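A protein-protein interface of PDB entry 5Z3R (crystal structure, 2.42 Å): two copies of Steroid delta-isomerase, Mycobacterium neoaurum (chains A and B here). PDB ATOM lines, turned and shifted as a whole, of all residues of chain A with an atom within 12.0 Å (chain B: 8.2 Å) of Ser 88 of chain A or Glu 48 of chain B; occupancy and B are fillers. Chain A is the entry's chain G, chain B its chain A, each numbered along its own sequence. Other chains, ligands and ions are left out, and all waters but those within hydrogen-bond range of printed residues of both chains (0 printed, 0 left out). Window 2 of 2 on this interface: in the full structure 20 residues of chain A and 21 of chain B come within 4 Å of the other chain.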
ATOM      1  N   SER A  11      16.890 -28.528  15.935  1.00  0.00           N
ATOM      2  CA  SER A  11      17.894 -28.148  14.849  1.00  0.00           C
ATOM      3  C   SER A  11      18.188 -29.326  13.853  1.00  0.00           C
ATOM      4  O   SER A  11      18.759 -30.339  14.267  1.00  0.00           O
ATOM      5  CB  SER A  11      19.208 -27.662  15.487  1.00  0.00           C
ATOM      6  OG  SER A  11      20.230 -27.514  14.495  1.00  0.00           O
ATOM      7  N   PRO A  12      17.832 -29.195  12.550  1.00  0.00           N
ATOM      8  CA  PRO A  12      17.820 -30.405  11.678  1.00  0.00           C
ATOM      9  C   PRO A  12      19.183 -31.169  11.515  1.00  0.00           C
ATOM     10  O   PRO A  12      19.216 -32.403  11.485  1.00  0.00           O
ATOM     11  CB  PRO A  12      17.282 -29.870  10.323  1.00  0.00           C
ATOM     12  CG  PRO A  12      17.444 -28.375  10.341  1.00  0.00           C
ATOM     13  CD  PRO A  12      17.692 -27.940  11.771  1.00  0.00           C
ATOM     14  N   VAL A  13      20.283 -30.433  11.480  1.00  0.00           N
ATOM     15  CA  VAL A  13      21.606 -31.029  11.357  1.00  0.00           C
ATOM     16  C   VAL A  13      22.063 -31.789  12.607  1.00  0.00           C
ATOM     17  O   VAL A  13      22.714 -32.832  12.490  1.00  0.00           O
ATOM     18  CB  VAL A  13      22.658 -29.969  10.950  1.00  0.00           C
ATOM     19  CG1 VAL A  13      23.210 -29.207  12.177  1.00  0.00           C
ATOM     20  CG2 VAL A  13      23.755 -30.617  10.108  1.00  0.00           C
ATOM     21  N   VAL A  14      21.723 -31.284  13.789  1.00  0.00           N
ATOM     22  CA  VAL A  14      21.989 -32.023  15.027  1.00  0.00           C
ATOM     23  C   VAL A  14      21.221 -33.329  15.112  1.00  0.00           C
ATOM     24  O   VAL A  14      21.792 -34.340  15.522  1.00  0.00           O
ATOM     25  CB  VAL A  14      21.714 -31.195  16.283  1.00  0.00           C
ATOM     26  CG1 VAL A  14      21.877 -32.060  17.544  1.00  0.00           C
ATOM     27  CG2 VAL A  14      22.636 -29.960  16.321  1.00  0.00           C
ATOM     28  N   THR A  84      31.727 -30.036  20.007  1.00  0.00           N
ATOM     29  CA  THR A  84      30.640 -29.647  19.115  1.00  0.00           C
ATOM     30  C   THR A  84      30.831 -28.207  18.721  1.00  0.00           C
ATOM     31  O   THR A  84      31.058 -27.374  19.573  1.00  0.00           O
ATOM     32  CB  THR A  84      29.291 -29.814  19.834  1.00  0.00           C
ATOM     33  OG1 THR A  84      29.240 -31.112  20.446  1.00  0.00           O
ATOM     34  CG2 THR A  84      28.138 -29.660  18.851  1.00  0.00           C
ATOM     35  N   PHE A  85      30.772 -27.908  17.431  1.00  0.00           N
ATOM     36  CA  PHE A  85      31.012 -26.548  16.946  1.00  0.00           C
ATOM     37  C   PHE A  85      29.886 -26.179  15.982  1.00  0.00           C
ATOM     38  O   PHE A  85      30.044 -26.359  14.752  1.00  0.00           O
ATOM     39  CB  PHE A  85      32.360 -26.446  16.242  1.00  0.00           C
ATOM     40  CG  PHE A  85      33.514 -26.797  17.109  1.00  0.00           C
ATOM     41  CD1 PHE A  85      33.964 -28.112  17.190  1.00  0.00           C
ATOM     42  CD2 PHE A  85      34.165 -25.824  17.843  1.00  0.00           C
ATOM     43  CE1 PHE A  85      35.034 -28.457  18.020  1.00  0.00           C
ATOM     44  CE2 PHE A  85      35.228 -26.156  18.683  1.00  0.00           C
ATOM     45  CZ  PHE A  85      35.676 -27.476  18.762  1.00  0.00           C
ATOM     46  N   PRO A  86      28.742 -25.674  16.531  1.00  0.00           N
ATOM     47  CA  PRO A  86      27.629 -25.255  15.693  1.00  0.00           C
ATOM     48  C   PRO A  86      28.087 -24.083  14.881  1.00  0.00           C
ATOM     49  O   PRO A  86      28.960 -23.326  15.326  1.00  0.00           O
ATOM     50  CB  PRO A  86      26.546 -24.823  16.706  1.00  0.00           C
ATOM     51  CG  PRO A  86      26.967 -25.372  18.032  1.00  0.00           C
ATOM     52  CD  PRO A  86      28.470 -25.346  17.949  1.00  0.00           C
ATOM     53  N   SER A  87      27.550 -23.970  13.673  1.00  0.00           N
ATOM     54  CA  SER A  87      27.735 -22.779  12.867  1.00  0.00           C
ATOM     55  C   SER A  87      26.605 -21.767  13.177  1.00  0.00           C
ATOM     56  O   SER A  87      25.763 -21.993  14.032  1.00  0.00           O
ATOM     57  CB  SER A  87      27.750 -23.168  11.384  1.00  0.00           C
ATOM     58  OG  SER A  87      26.611 -23.929  11.055  1.00  0.00           O
ATOM     59  N   SER A  88      26.598 -20.645  12.481  1.00  0.00           N
ATOM     60  CA  SER A  88      25.435 -19.780  12.478  1.00  0.00           C
ATOM     61  C   SER A  88      24.403 -20.197  11.419  1.00  0.00           C
ATOM     62  O   SER A  88      23.556 -19.393  11.086  1.00  0.00           O
ATOM     63  CB  SER A  88      25.870 -18.365  12.231  1.00  0.00           C
ATOM     64  OG  SER A  88      26.811 -17.999  13.179  1.00  0.00           O
ATOM     65  N   SER A  89      24.513 -21.408  10.846  1.00  0.00           N
ATOM     66  CA  SER A  89      23.460 -22.003  10.035  1.00  0.00           C
ATOM     67  C   SER A  89      22.937 -23.255  10.739  1.00  0.00           C
ATOM     68  O   SER A  89      23.697 -23.988  11.362  1.00  0.00           O
ATOM     69  CB  SER A  89      23.955 -22.350   8.636  1.00  0.00           C
ATOM     70  OG  SER A  89      22.994 -23.126   7.929  1.00  0.00           O
ATOM     71  N   PRO A  90      21.622 -23.482  10.677  1.00  0.00           N
ATOM     72  CA  PRO A  90      21.048 -24.685  11.292  1.00  0.00           C
ATOM     73  C   PRO A  90      21.181 -25.960  10.427  1.00  0.00           C
ATOM     74  O   PRO A  90      20.894 -27.074  10.884  1.00  0.00           O
ATOM     75  CB  PRO A  90      19.586 -24.290  11.481  1.00  0.00           C
ATOM     76  CG  PRO A  90      19.320 -23.305  10.383  1.00  0.00           C
ATOM     77  CD  PRO A  90      20.581 -22.531  10.225  1.00  0.00           C
ATOM     78  N   THR A  91      21.619 -25.804   9.186  1.00  0.00           N
ATOM     79  CA  THR A  91      21.820 -26.937   8.322  1.00  0.00           C
ATOM     80  C   THR A  91      23.229 -27.522   8.348  1.00  0.00           C
ATOM     81  O   THR A  91      23.418 -28.593   7.793  1.00  0.00           O
ATOM     82  CB  THR A  91      21.538 -26.534   6.889  1.00  0.00           C
ATOM     83  OG1 THR A  91      22.306 -25.363   6.590  1.00  0.00           O
ATOM     84  CG2 THR A  91      20.013 -26.307   6.690  1.00  0.00           C
ATOM     85  N   GLU A  92      24.197 -26.847   8.984  1.00  0.00           N
ATOM     86  CA  GLU A  92      25.616 -27.278   8.983  1.00  0.00           C
ATOM     87  C   GLU A  92      26.314 -27.197  10.350  1.00  0.00           C
ATOM     88  O   GLU A  92      26.378 -26.143  10.990  1.00  0.00           O
ATOM     89  CB  GLU A  92      26.423 -26.485   7.941  1.00  0.00           C
ATOM     90  CG  GLU A  92      25.945 -26.741   6.512  1.00  0.00           C
ATOM     91  CD  GLU A  92      26.915 -26.250   5.447  1.00  0.00           C
ATOM     92  OE1 GLU A  92      26.742 -25.122   4.965  1.00  0.00           O
ATOM     93  OE2 GLU A  92      27.848 -26.999   5.065  1.00  0.00           O
ATOM     94  N   ILE A  93      26.861 -28.319  10.771  1.00  0.00           N
ATOM     95  CA  ILE A  93      27.623 -28.386  12.007  1.00  0.00           C
ATOM     96  C   ILE A  93      28.974 -29.150  11.800  1.00  0.00           C
ATOM     97  O   ILE A  93      29.171 -29.848  10.809  1.00  0.00           O
ATOM     98  CB  ILE A  93      26.745 -29.025  13.088  1.00  0.00           C
ATOM     99  CG1 ILE A  93      27.336 -28.833  14.487  1.00  0.00           C
ATOM    100  CG2 ILE A  93      26.527 -30.509  12.819  1.00  0.00           C
ATOM    101  CD1 ILE A  93      26.386 -29.197  15.610  1.00  0.00           C
ATOM    102  N   ALA A  94      29.905 -28.966  12.727  1.00  0.00           N
ATOM    103  CA  ALA A  94      31.186 -29.678  12.759  1.00  0.00           C
ATOM    104  C   ALA A  94      31.367 -30.248  14.138  1.00  0.00           C
ATOM    105  O   ALA A  94      31.076 -29.561  15.120  1.00  0.00           O
ATOM    106  CB  ALA A  94      32.346 -28.728  12.443  1.00  0.00           C
ATOM    107  N   TYR A 117      28.960 -32.112   8.949  1.00  0.00           N
ATOM    108  CA  TYR A 117      27.662 -32.547   8.403  1.00  0.00           C
ATOM    109  C   TYR A 117      26.924 -31.379   7.765  1.00  0.00           C
ATOM    110  O   TYR A 117      27.157 -30.230   8.116  1.00  0.00           O
ATOM    111  CB  TYR A 117      26.777 -33.155   9.481  1.00  0.00           C
ATOM    112  CG  TYR A 117      27.288 -34.451  10.092  1.00  0.00           C
ATOM    113  CD1 TYR A 117      28.305 -34.461  11.045  1.00  0.00           C
ATOM    114  CD2 TYR A 117      26.718 -35.675   9.757  1.00  0.00           C
ATOM    115  CE1 TYR A 117      28.740 -35.657  11.636  1.00  0.00           C
ATOM    116  CE2 TYR A 117      27.159 -36.861  10.338  1.00  0.00           C
ATOM    117  CZ  TYR A 117      28.167 -36.841  11.267  1.00  0.00           C
ATOM    118  OH  TYR A 117      28.569 -38.025  11.824  1.00  0.00           O
ATOM    119  N   ARG A 118      26.084 -31.698   6.779  1.00  0.00           N
ATOM    120  CA  ARG A 118      25.192 -30.748   6.099  1.00  0.00           C
ATOM    121  C   ARG A 118      23.863 -31.436   5.757  1.00  0.00           C
ATOM    122  O   ARG A 118      23.845 -32.577   5.267  1.00  0.00           O
ATOM    123  CB  ARG A 118      25.821 -30.214   4.819  1.00  0.00           C
ATOM    124  CG  ARG A 118      24.941 -29.273   3.994  1.00  0.00           C
ATOM    125  CD  ARG A 118      25.747 -28.689   2.828  1.00  0.00           C
ATOM    126  NE  ARG A 118      25.030 -27.664   2.060  1.00  0.00           N
ATOM    127  CZ  ARG A 118      23.961 -27.887   1.280  1.00  0.00           C
ATOM    128  NH1 ARG A 118      23.430 -29.102   1.124  1.00  0.00           N
ATOM    129  NH2 ARG A 118      23.406 -26.882   0.646  1.00  0.00           N
ATOM    130  N   VAL A 119      22.753 -30.738   5.996  1.00  0.00           N
ATOM    131  CA  VAL A 119      21.437 -31.226   5.546  1.00  0.00           C
ATOM    132  C   VAL A 119      20.870 -30.324   4.431  1.00  0.00           C
ATOM    133  O   VAL A 119      21.278 -29.141   4.304  1.00  0.00           O
ATOM    134  CB  VAL A 119      20.453 -31.380   6.720  1.00  0.00           C
ATOM    135  CG1 VAL A 119      20.930 -32.458   7.681  1.00  0.00           C
ATOM    136  CG2 VAL A 119      20.253 -30.060   7.460  1.00  0.00           C
ATOM    137  N   ASP B  44      32.913 -16.878   6.831  1.00  0.00           N
ATOM    138  CA  ASP B  44      33.299 -16.691   8.199  1.00  0.00           C
ATOM    139  C   ASP B  44      32.163 -15.962   8.965  1.00  0.00           C
ATOM    140  O   ASP B  44      32.065 -14.736   8.925  1.00  0.00           O
ATOM    141  CB  ASP B  44      34.613 -15.923   8.236  1.00  0.00           C
ATOM    142  CG  ASP B  44      35.237 -15.914   9.604  1.00  0.00           C
ATOM    143  OD1 ASP B  44      34.822 -16.744  10.462  1.00  0.00           O
ATOM    144  OD2 ASP B  44      36.141 -15.069   9.820  1.00  0.00           O
ATOM    145  N   PRO B  45      31.277 -16.681   9.638  1.00  0.00           N
ATOM    146  CA  PRO B  45      31.157 -18.118   9.660  1.00  0.00           C
ATOM    147  C   PRO B  45      30.204 -18.540   8.591  1.00  0.00           C
ATOM    148  O   PRO B  45      29.832 -17.722   7.736  1.00  0.00           O
ATOM    149  CB  PRO B  45      30.505 -18.365  11.026  1.00  0.00           C
ATOM    150  CG  PRO B  45      29.625 -17.195  11.213  1.00  0.00           C
ATOM    151  CD  PRO B  45      30.232 -16.048  10.448  1.00  0.00           C
ATOM    152  N   ILE B  46      29.829 -19.811   8.641  1.00  0.00           N
ATOM    153  CA  ILE B  46      28.781 -20.362   7.811  1.00  0.00           C
ATOM    154  C   ILE B  46      27.449 -19.934   8.419  1.00  0.00           C
ATOM    155  O   ILE B  46      27.231 -20.040   9.644  1.00  0.00           O
ATOM    156  CB  ILE B  46      28.839 -21.925   7.771  1.00  0.00           C
ATOM    157  CG1 ILE B  46      30.174 -22.416   7.154  1.00  0.00           C
ATOM    158  CG2 ILE B  46      27.628 -22.493   7.009  1.00  0.00           C
ATOM    159  CD1 ILE B  46      30.550 -23.868   7.462  1.00  0.00           C
ATOM    160  N   GLY B  47      26.531 -19.521   7.555  1.00  0.00           N
ATOM    161  CA  GLY B  47      25.229 -19.024   8.002  1.00  0.00           C
ATOM    162  C   GLY B  47      25.220 -17.532   8.255  1.00  0.00           C
ATOM    163  O   GLY B  47      26.276 -16.867   8.206  1.00  0.00           O
ATOM    164  N   GLU B  48      24.017 -16.997   8.481  1.00  0.00           N
ATOM    165  CA  GLU B  48      23.839 -15.548   8.607  1.00  0.00           C
ATOM    166  C   GLU B  48      24.427 -15.076   9.927  1.00  0.00           C
ATOM    167  O   GLU B  48      24.124 -15.631  11.000  1.00  0.00           O
ATOM    168  CB  GLU B  48      22.369 -15.148   8.497  1.00  0.00           C
ATOM    169  CG  GLU B  48      21.802 -15.335   7.091  1.00  0.00           C
ATOM    170  CD  GLU B  48      20.323 -14.975   6.956  1.00  0.00           C
ATOM    171  OE1 GLU B  48      19.728 -14.407   7.911  1.00  0.00           O
ATOM    172  OE2 GLU B  48      19.763 -15.267   5.871  1.00  0.00           O
ATOM    173  N   ALA B  49      25.310 -14.083   9.829  1.00  0.00           N
ATOM    174  CA  ALA B  49      25.898 -13.430  10.993  1.00  0.00           C
ATOM    175  C   ALA B  49      26.524 -12.067  10.619  1.00  0.00           C
ATOM    176  O   ALA B  49      26.526 -11.649   9.470  1.00  0.00           O
ATOM    177  CB  ALA B  49      26.924 -14.344  11.668  1.00  0.00           C
ATOM    178  N   VAL B  50      27.056 -11.389  11.621  1.00  0.00           N
ATOM    179  CA  VAL B  50      27.578 -10.026  11.499  1.00  0.00           C
ATOM    180  C   VAL B  50      28.559  -9.835  10.340  1.00  0.00           C
ATOM    181  O   VAL B  50      28.605  -8.775   9.709  1.00  0.00           O
ATOM    182  CB  VAL B  50      28.255  -9.628  12.841  1.00  0.00           C
ATOM    183  CG1 VAL B  50      29.107  -8.370  12.699  1.00  0.00           C
ATOM    184  CG2 VAL B  50      27.194  -9.454  13.937  1.00  0.00           C
ATOM    185  N   THR B  51      29.347 -10.878  10.101  1.00  0.00           N
ATOM    186  CA  THR B  51      30.396 -10.898   9.082  1.00  0.00           C
ATOM    187  C   THR B  51      30.037 -11.803   7.838  1.00  0.00           C
ATOM    188  O   THR B  51      30.773 -11.833   6.831  1.00  0.00           O
ATOM    189  CB  THR B  51      31.763 -11.246   9.728  1.00  0.00           C
ATOM    190  OG1 THR B  51      32.568 -11.956   8.785  1.00  0.00           O
ATOM    191  CG2 THR B  51      31.634 -12.102  10.974  1.00  0.00           C
ATOM    192  N   ASN B  52      28.918 -12.533   7.927  1.00  0.00           N
ATOM    193  CA  ASN B  52      28.242 -13.153   6.772  1.00  0.00           C
ATOM    194  C   ASN B  52      26.751 -12.672   6.715  1.00  0.00           C
ATOM    195  O   ASN B  52      25.812 -13.437   7.034  1.00  0.00           O
ATOM    196  CB  ASN B  52      28.371 -14.684   6.863  1.00  0.00           C
ATOM    197  CG  ASN B  52      27.931 -15.400   5.595  1.00  0.00           C
ATOM    198  OD1 ASN B  52      27.598 -14.756   4.584  1.00  0.00           O
ATOM    199  ND2 ASN B  52      27.944 -16.747   5.631  1.00  0.00           N
ATOM    200  N   PRO B  53      26.536 -11.390   6.335  1.00  0.00           N
ATOM    201  CA  PRO B  53      25.173 -10.796   6.399  1.00  0.00           C
ATOM    202  C   PRO B  53      24.155 -11.546   5.490  1.00  0.00           C
ATOM    203  O   PRO B  53      23.164 -12.097   5.967  1.00  0.00           O
ATOM    204  CB  PRO B  53      25.404  -9.330   5.962  1.00  0.00           C
ATOM    205  CG  PRO B  53      26.716  -9.305   5.226  1.00  0.00           C
ATOM    206  CD  PRO B  53      27.522 -10.493   5.684  1.00  0.00           C
ATOM    207  N   ASP B  54      24.433 -11.513   4.194  1.00  0.00           N
ATOM    208  CA  ASP B  54      24.036 -12.490   3.176  1.00  0.00           C
ATOM    209  C   ASP B  54      23.636 -13.929   3.612  1.00  0.00           C
ATOM    210  O   ASP B  54      22.698 -14.500   3.051  1.00  0.00           O
ATOM    211  CB  ASP B  54      25.249 -12.569   2.196  1.00  0.00           C
ATOM    212  CG  ASP B  54      24.910 -13.151   0.820  1.00  0.00           C
ATOM    213  OD1 ASP B  54      23.720 -13.271   0.468  1.00  0.00           O
ATOM    214  OD2 ASP B  54      25.871 -13.489   0.079  1.00  0.00           O
ATOM    215  N   GLY B  55      24.395 -14.549   4.524  1.00  0.00           N
ATOM    216  CA  GLY B  55      24.269 -16.003   4.822  1.00  0.00           C
ATOM    217  C   GLY B  55      24.896 -16.998   3.824  1.00  0.00           C
ATOM    218  O   GLY B  55      24.957 -18.199   4.105  1.00  0.00           O
ATOM    219  N   THR B  56      25.340 -16.504   2.667  1.00  0.00           N
ATOM    220  CA  THR B  56      25.899 -17.310   1.556  1.00  0.00           C
ATOM    221  C   THR B  56      27.347 -16.889   1.182  1.00  0.00           C
ATOM    222  O   THR B  56      27.825 -17.177   0.076  1.00  0.00           O
ATOM    223  CB  THR B  56      25.020 -17.177   0.279  1.00  0.00           C
ATOM    224  OG1 THR B  56      25.335 -15.953  -0.417  1.00  0.00           O
ATOM    225  CG2 THR B  56      23.512 -17.216   0.632  1.00  0.00           C
ATOM    226  N   GLY B  57      28.010 -16.148   2.067  1.00  0.00           N
ATOM    227  CA  GLY B  57      29.432 -15.923   1.990  1.00  0.00           C
ATOM    228  C   GLY B  57      29.826 -14.850   1.027  1.00  0.00           C
ATOM    229  O   GLY B  57      29.051 -14.457   0.158  1.00  0.00           O
ATOM    230  N   GLY B 130      33.994 -21.302   8.426  1.00  0.00           N
ATOM    231  CA  GLY B 130      34.090 -21.179   9.894  1.00  0.00           C
ATOM    232  C   GLY B 130      32.838 -21.724  10.563  1.00  0.00           C
ATOM    233  O   GLY B 130      31.717 -21.329  10.230  1.00  0.00           O
ATOM    234  N   TYR B 131      33.038 -22.664  11.473  1.00  0.00           N
ATOM    235  CA  TYR B 131      31.964 -23.223  12.268  1.00  0.00           C
ATOM    236  C   TYR B 131      31.962 -22.550  13.659  1.00  0.00           C
ATOM    237  O   TYR B 131      32.683 -22.991  14.577  1.00  0.00           O
ATOM    238  CB  TYR B 131      32.091 -24.748  12.392  1.00  0.00           C
ATOM    239  CG  TYR B 131      31.876 -25.529  11.130  1.00  0.00           C
ATOM    240  CD1 TYR B 131      32.881 -25.631  10.171  1.00  0.00           C
ATOM    241  CD2 TYR B 131      30.681 -26.199  10.890  1.00  0.00           C
ATOM    242  CE1 TYR B 131      32.681 -26.335   8.988  1.00  0.00           C
ATOM    243  CE2 TYR B 131      30.486 -26.917   9.714  1.00  0.00           C
ATOM    244  CZ  TYR B 131      31.502 -26.973   8.769  1.00  0.00           C
ATOM    245  OH  TYR B 131      31.354 -27.679   7.627  1.00  0.00           O
ATOM    246  N   TRP B 132      31.151 -21.486  13.770  1.00  0.00           N
ATOM    247  CA  TRP B 132      30.876 -20.736  15.003  1.00  0.00           C
ATOM    248  C   TRP B 132      29.630 -19.830  14.890  1.00  0.00           C
ATOM    249  O   TRP B 132      29.176 -19.507  13.781  1.00  0.00           O
ATOM    250  CB  TRP B 132      32.069 -19.864  15.372  1.00  0.00           C
ATOM    251  CG  TRP B 132      32.493 -18.787  14.375  1.00  0.00           C
ATOM    252  CD1 TRP B 132      33.446 -18.910  13.429  1.00  0.00           C
ATOM    253  CD2 TRP B 132      32.066 -17.421  14.322  1.00  0.00           C
ATOM    254  NE1 TRP B 132      33.618 -17.733  12.752  1.00  0.00           N
ATOM    255  CE2 TRP B 132      32.790 -16.795  13.282  1.00  0.00           C
ATOM    256  CE3 TRP B 132      31.124 -16.665  15.027  1.00  0.00           C
ATOM    257  CZ2 TRP B 132      32.616 -15.433  12.934  1.00  0.00           C
ATOM    258  CZ3 TRP B 132      30.942 -15.280  14.669  1.00  0.00           C
ATOM    259  CH2 TRP B 132      31.691 -14.697  13.641  1.00  0.00           C
ATOM    260  N   ASN B 133      29.103 -19.417  16.043  1.00  0.00           N
ATOM    261  CA  ASN B 133      28.036 -18.382  16.115  1.00  0.00           C
ATOM    262  C   ASN B 133      28.308 -17.369  17.195  1.00  0.00           C
ATOM    263  O   ASN B 133      29.284 -17.486  17.944  1.00  0.00           O
ATOM    264  CB  ASN B 133      26.618 -18.977  16.286  1.00  0.00           C
ATOM    265  CG  ASN B 133      26.546 -20.067  17.344  1.00  0.00           C
ATOM    266  OD1 ASN B 133      26.932 -19.890  18.502  1.00  0.00           O
ATOM    267  ND2 ASN B 133      26.054 -21.219  16.931  1.00  0.00           N
ATOM    268  N   MET B 134      27.446 -16.353  17.239  1.00  0.00           N
ATOM    269  CA  MET B 134      27.526 -15.266  18.208  1.00  0.00           C
ATOM    270  C   MET B 134      27.428 -15.761  19.646  1.00  0.00           C
ATOM    271  O   MET B 134      28.127 -15.240  20.492  1.00  0.00           O
ATOM    272  CB  MET B 134      26.448 -14.234  17.901  1.00  0.00           C
ATOM    273  CG  MET B 134      26.661 -13.526  16.565  1.00  0.00           C
ATOM    274  SD  MET B 134      28.128 -12.476  16.593  1.00  0.00           S
ATOM    275  CE  MET B 134      27.756 -11.427  18.009  1.00  0.00           C
ATOM    276  N   ASP B 135      26.640 -16.813  19.904  1.00  0.00           N
ATOM    277  CA  ASP B 135      26.605 -17.485  21.245  1.00  0.00           C
ATOM    278  C   ASP B 135      27.966 -17.887  21.830  1.00  0.00           C
ATOM    279  O   ASP B 135      28.058 -18.104  23.049  1.00  0.00           O
ATOM    280  CB  ASP B 135      25.677 -18.753  21.271  1.00  0.00           C
ATOM    281  CG  ASP B 135      24.236 -18.436  21.689  1.00  0.00           C
ATOM    282  OD1 ASP B 135      23.771 -18.938  22.754  1.00  0.00           O
ATOM    283  OD2 ASP B 135      23.578 -17.672  20.941  1.00  0.00           O
ATOM    284  N   ALA B 136      28.975 -18.063  20.965  1.00  0.00           N
ATOM    285  CA  ALA B 136      30.350 -18.450  21.364  1.00  0.00           C
ATOM    286  C   ALA B 136      31.350 -17.270  21.417  1.00  0.00           C
ATOM    287  O   ALA B 136      32.365 -17.363  22.115  1.00  0.00           O
ATOM    288  CB  ALA B 136      30.883 -19.556  20.439  1.00  0.00           C
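Ser 88 of chain A touches just these residues of chain B: Pro 45 (3.5 Å), Ile 46 (3.0 Å), Gly 47 (3.5 Å), Glu 48 (3.5 Å), Ala 49 (3.96 Å), Trp 132 (2.9 Å) and Asn 133 (3.2 Å).
Of chain A, only Ser 88 comes within 4 Å of Glu 48 of chain B.
Ser 87 of chain A touches three residues of chain B.
Of chain A, only Ser 88 (3.5 Å) comes within 4 Å of Pro 45 of chain B.
Ile 46 of chain B touches just these residues of chain A: Ser 87 (3.6 Å), Ser 88 (3.0 Å), Ser 89 (3.3 Å) and Glu 92 (3.4 Å).
Gly 47 of chain B touches just these residues of chain A: Ser 88 and Ser 89.
No residue of chain A comes within 4 Å of Asn 52 of chain B.
No residue of chain A comes within 4 Å of Pro 53 of chain B.
Asn 133 of chain B touches just these residues of chain A: Pro 86, Ser 87 and Ser 88.
Of the printed residues of chain B, Ser 89 of chain A touches Ile 46 and Gly 47.
Printed residues of chain B within 4 Å of Pro 86 of chain A: Tyr 131 (3.5 Å), Trp 132 (3.2 Å) and Asn 133 (3.6 Å).
Of the printed residues of chain A, Tyr 131 of chain B touches Phe 85 (3.5 Å), Pro 86 (3.5 Å), Ile 93 (3.4 Å) and Ala 94 (3.4 Å).
Of the printed residues of chain B, Ile 93 of chain A touches Tyr 131.
Asp 54 of chain B touches none of the printed residues of chain A.
The nearest printed residue of chain B that does not touch Glu 92 of chain A is Tyr 131 of chain B (4.2 Å).
The backbone NH (N) of Ser 88 of chain A sits at hydrogen-bond distance from the backbone carbonyl oxygen (O) of Ile 46 of chain B, 3.0 Å away.
The backbone NH (N) of Ser 89 of chain A is in hydrogen-bond range of the backbone carbonyl oxygen (O) of Ile 46 of chain B, at 3.3 Å.
The backbone carbonyl oxygen (O) of Pro 86 of chain A sits close to the backbone NH (N) of Trp 132 of chain B, 3.3 Å away.
The side-chain hydroxyl (OG) of Ser 88 of chain A lies within hydrogen-bond range of the backbone carbonyl oxygen (O) of Trp 132 of chain B (2.9 Å).
ND2 of Asn 133 of chain B sits at hydrogen-bond distance from O of Ser 87 of chain A.
No position is printed for both chains.
Of the 19 pairs that touch across the chains among the printed residues, none has its exchanged pair printed and touching as well.
Among the printed residues, merely in contact across the chains: Phe 85 of chain A with Tyr 131 of chain B (3.5 Å), Pro 86 of chain A with Tyr 131 of chain B (3.5 Å), Pro 86 of chain A with Asn 133 of chain B (3.6 Å), Ser 87 of chain A with Ile 46 of chain B (3.6 Å), Ser 87 of chain A with Trp 132 of chain B (3.5 Å), Ser 88 of chain A with Pro 45 of chain B (3.5 Å), Ser 88 of chain A with Gly 47 of chain B (3.5 Å), Ser 88 of chain A with Glu 48 of chain B (3.5 Å), Ser 88 of chain A with Ala 49 of chain B (3.96 Å), Ser 88 of chain A with Asn 133 of chain B (3.2 Å), Ser 89 of chain A with Gly 47 of chain B (3.6 Å), Glu 92 of chain A with Ile 46 of chain B (3.4 Å), Ile 93 of chain A with Tyr 131 of chain B (3.4 Å) and Ala 94 of chain A with Tyr 131 of chain B (3.4 Å).
The side-chain amide nitrogen (ND2) of Asn 52 of chain B lies within hydrogen-bond range of the backbone carbonyl oxygen (O) of Pro 45 of chain B.
N of Ile 46 of chain B is in hydrogen-bond range of O of Gly 130 of chain B (2.9 Å).
O of Gly 47 of chain B sits at hydrogen-bond distance from ND2 of Asn 52 of chain B, 3.1 Å away.
The side-chain amide oxygen (OD1) of Asn 133 of chain B sits close to the backbone NH (N) of Asp 135 of chain B (3.4 Å).
The backbone NH (N) of Phe 85 of chain A lies within hydrogen-bond range of the backbone carbonyl oxygen (O) of Ala 94 of chain A, at 2.9 Å.
O of Ser 89 of chain A sits at hydrogen-bond distance from OG of Ser 87 of chain A, at 2.9 Å.
Of the 18 printed residues of chain A, 8 touch a printed residue of chain B.
Printed residues of chain A that touch a printed residue of chain B: Phe 85, Pro 86, Ser 87, Ser 88, Ser 89, Glu 92, Ile 93 and Ala 94.
Hydrophobic or aromatic side chains of chain B that line the printed part of chain A: Pro 45, Ile 46, Ala 49 and Tyr 131.
Along chain B the printed residues that touch a printed residue of chain A span positions 45 to 133.
Among the printed residues, 19 pairs touch across the chains.
Among the printed residues, no Asp or Glu carboxylate lies within 4 Å of a Lys or Arg side-chain nitrogen of the other chain.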
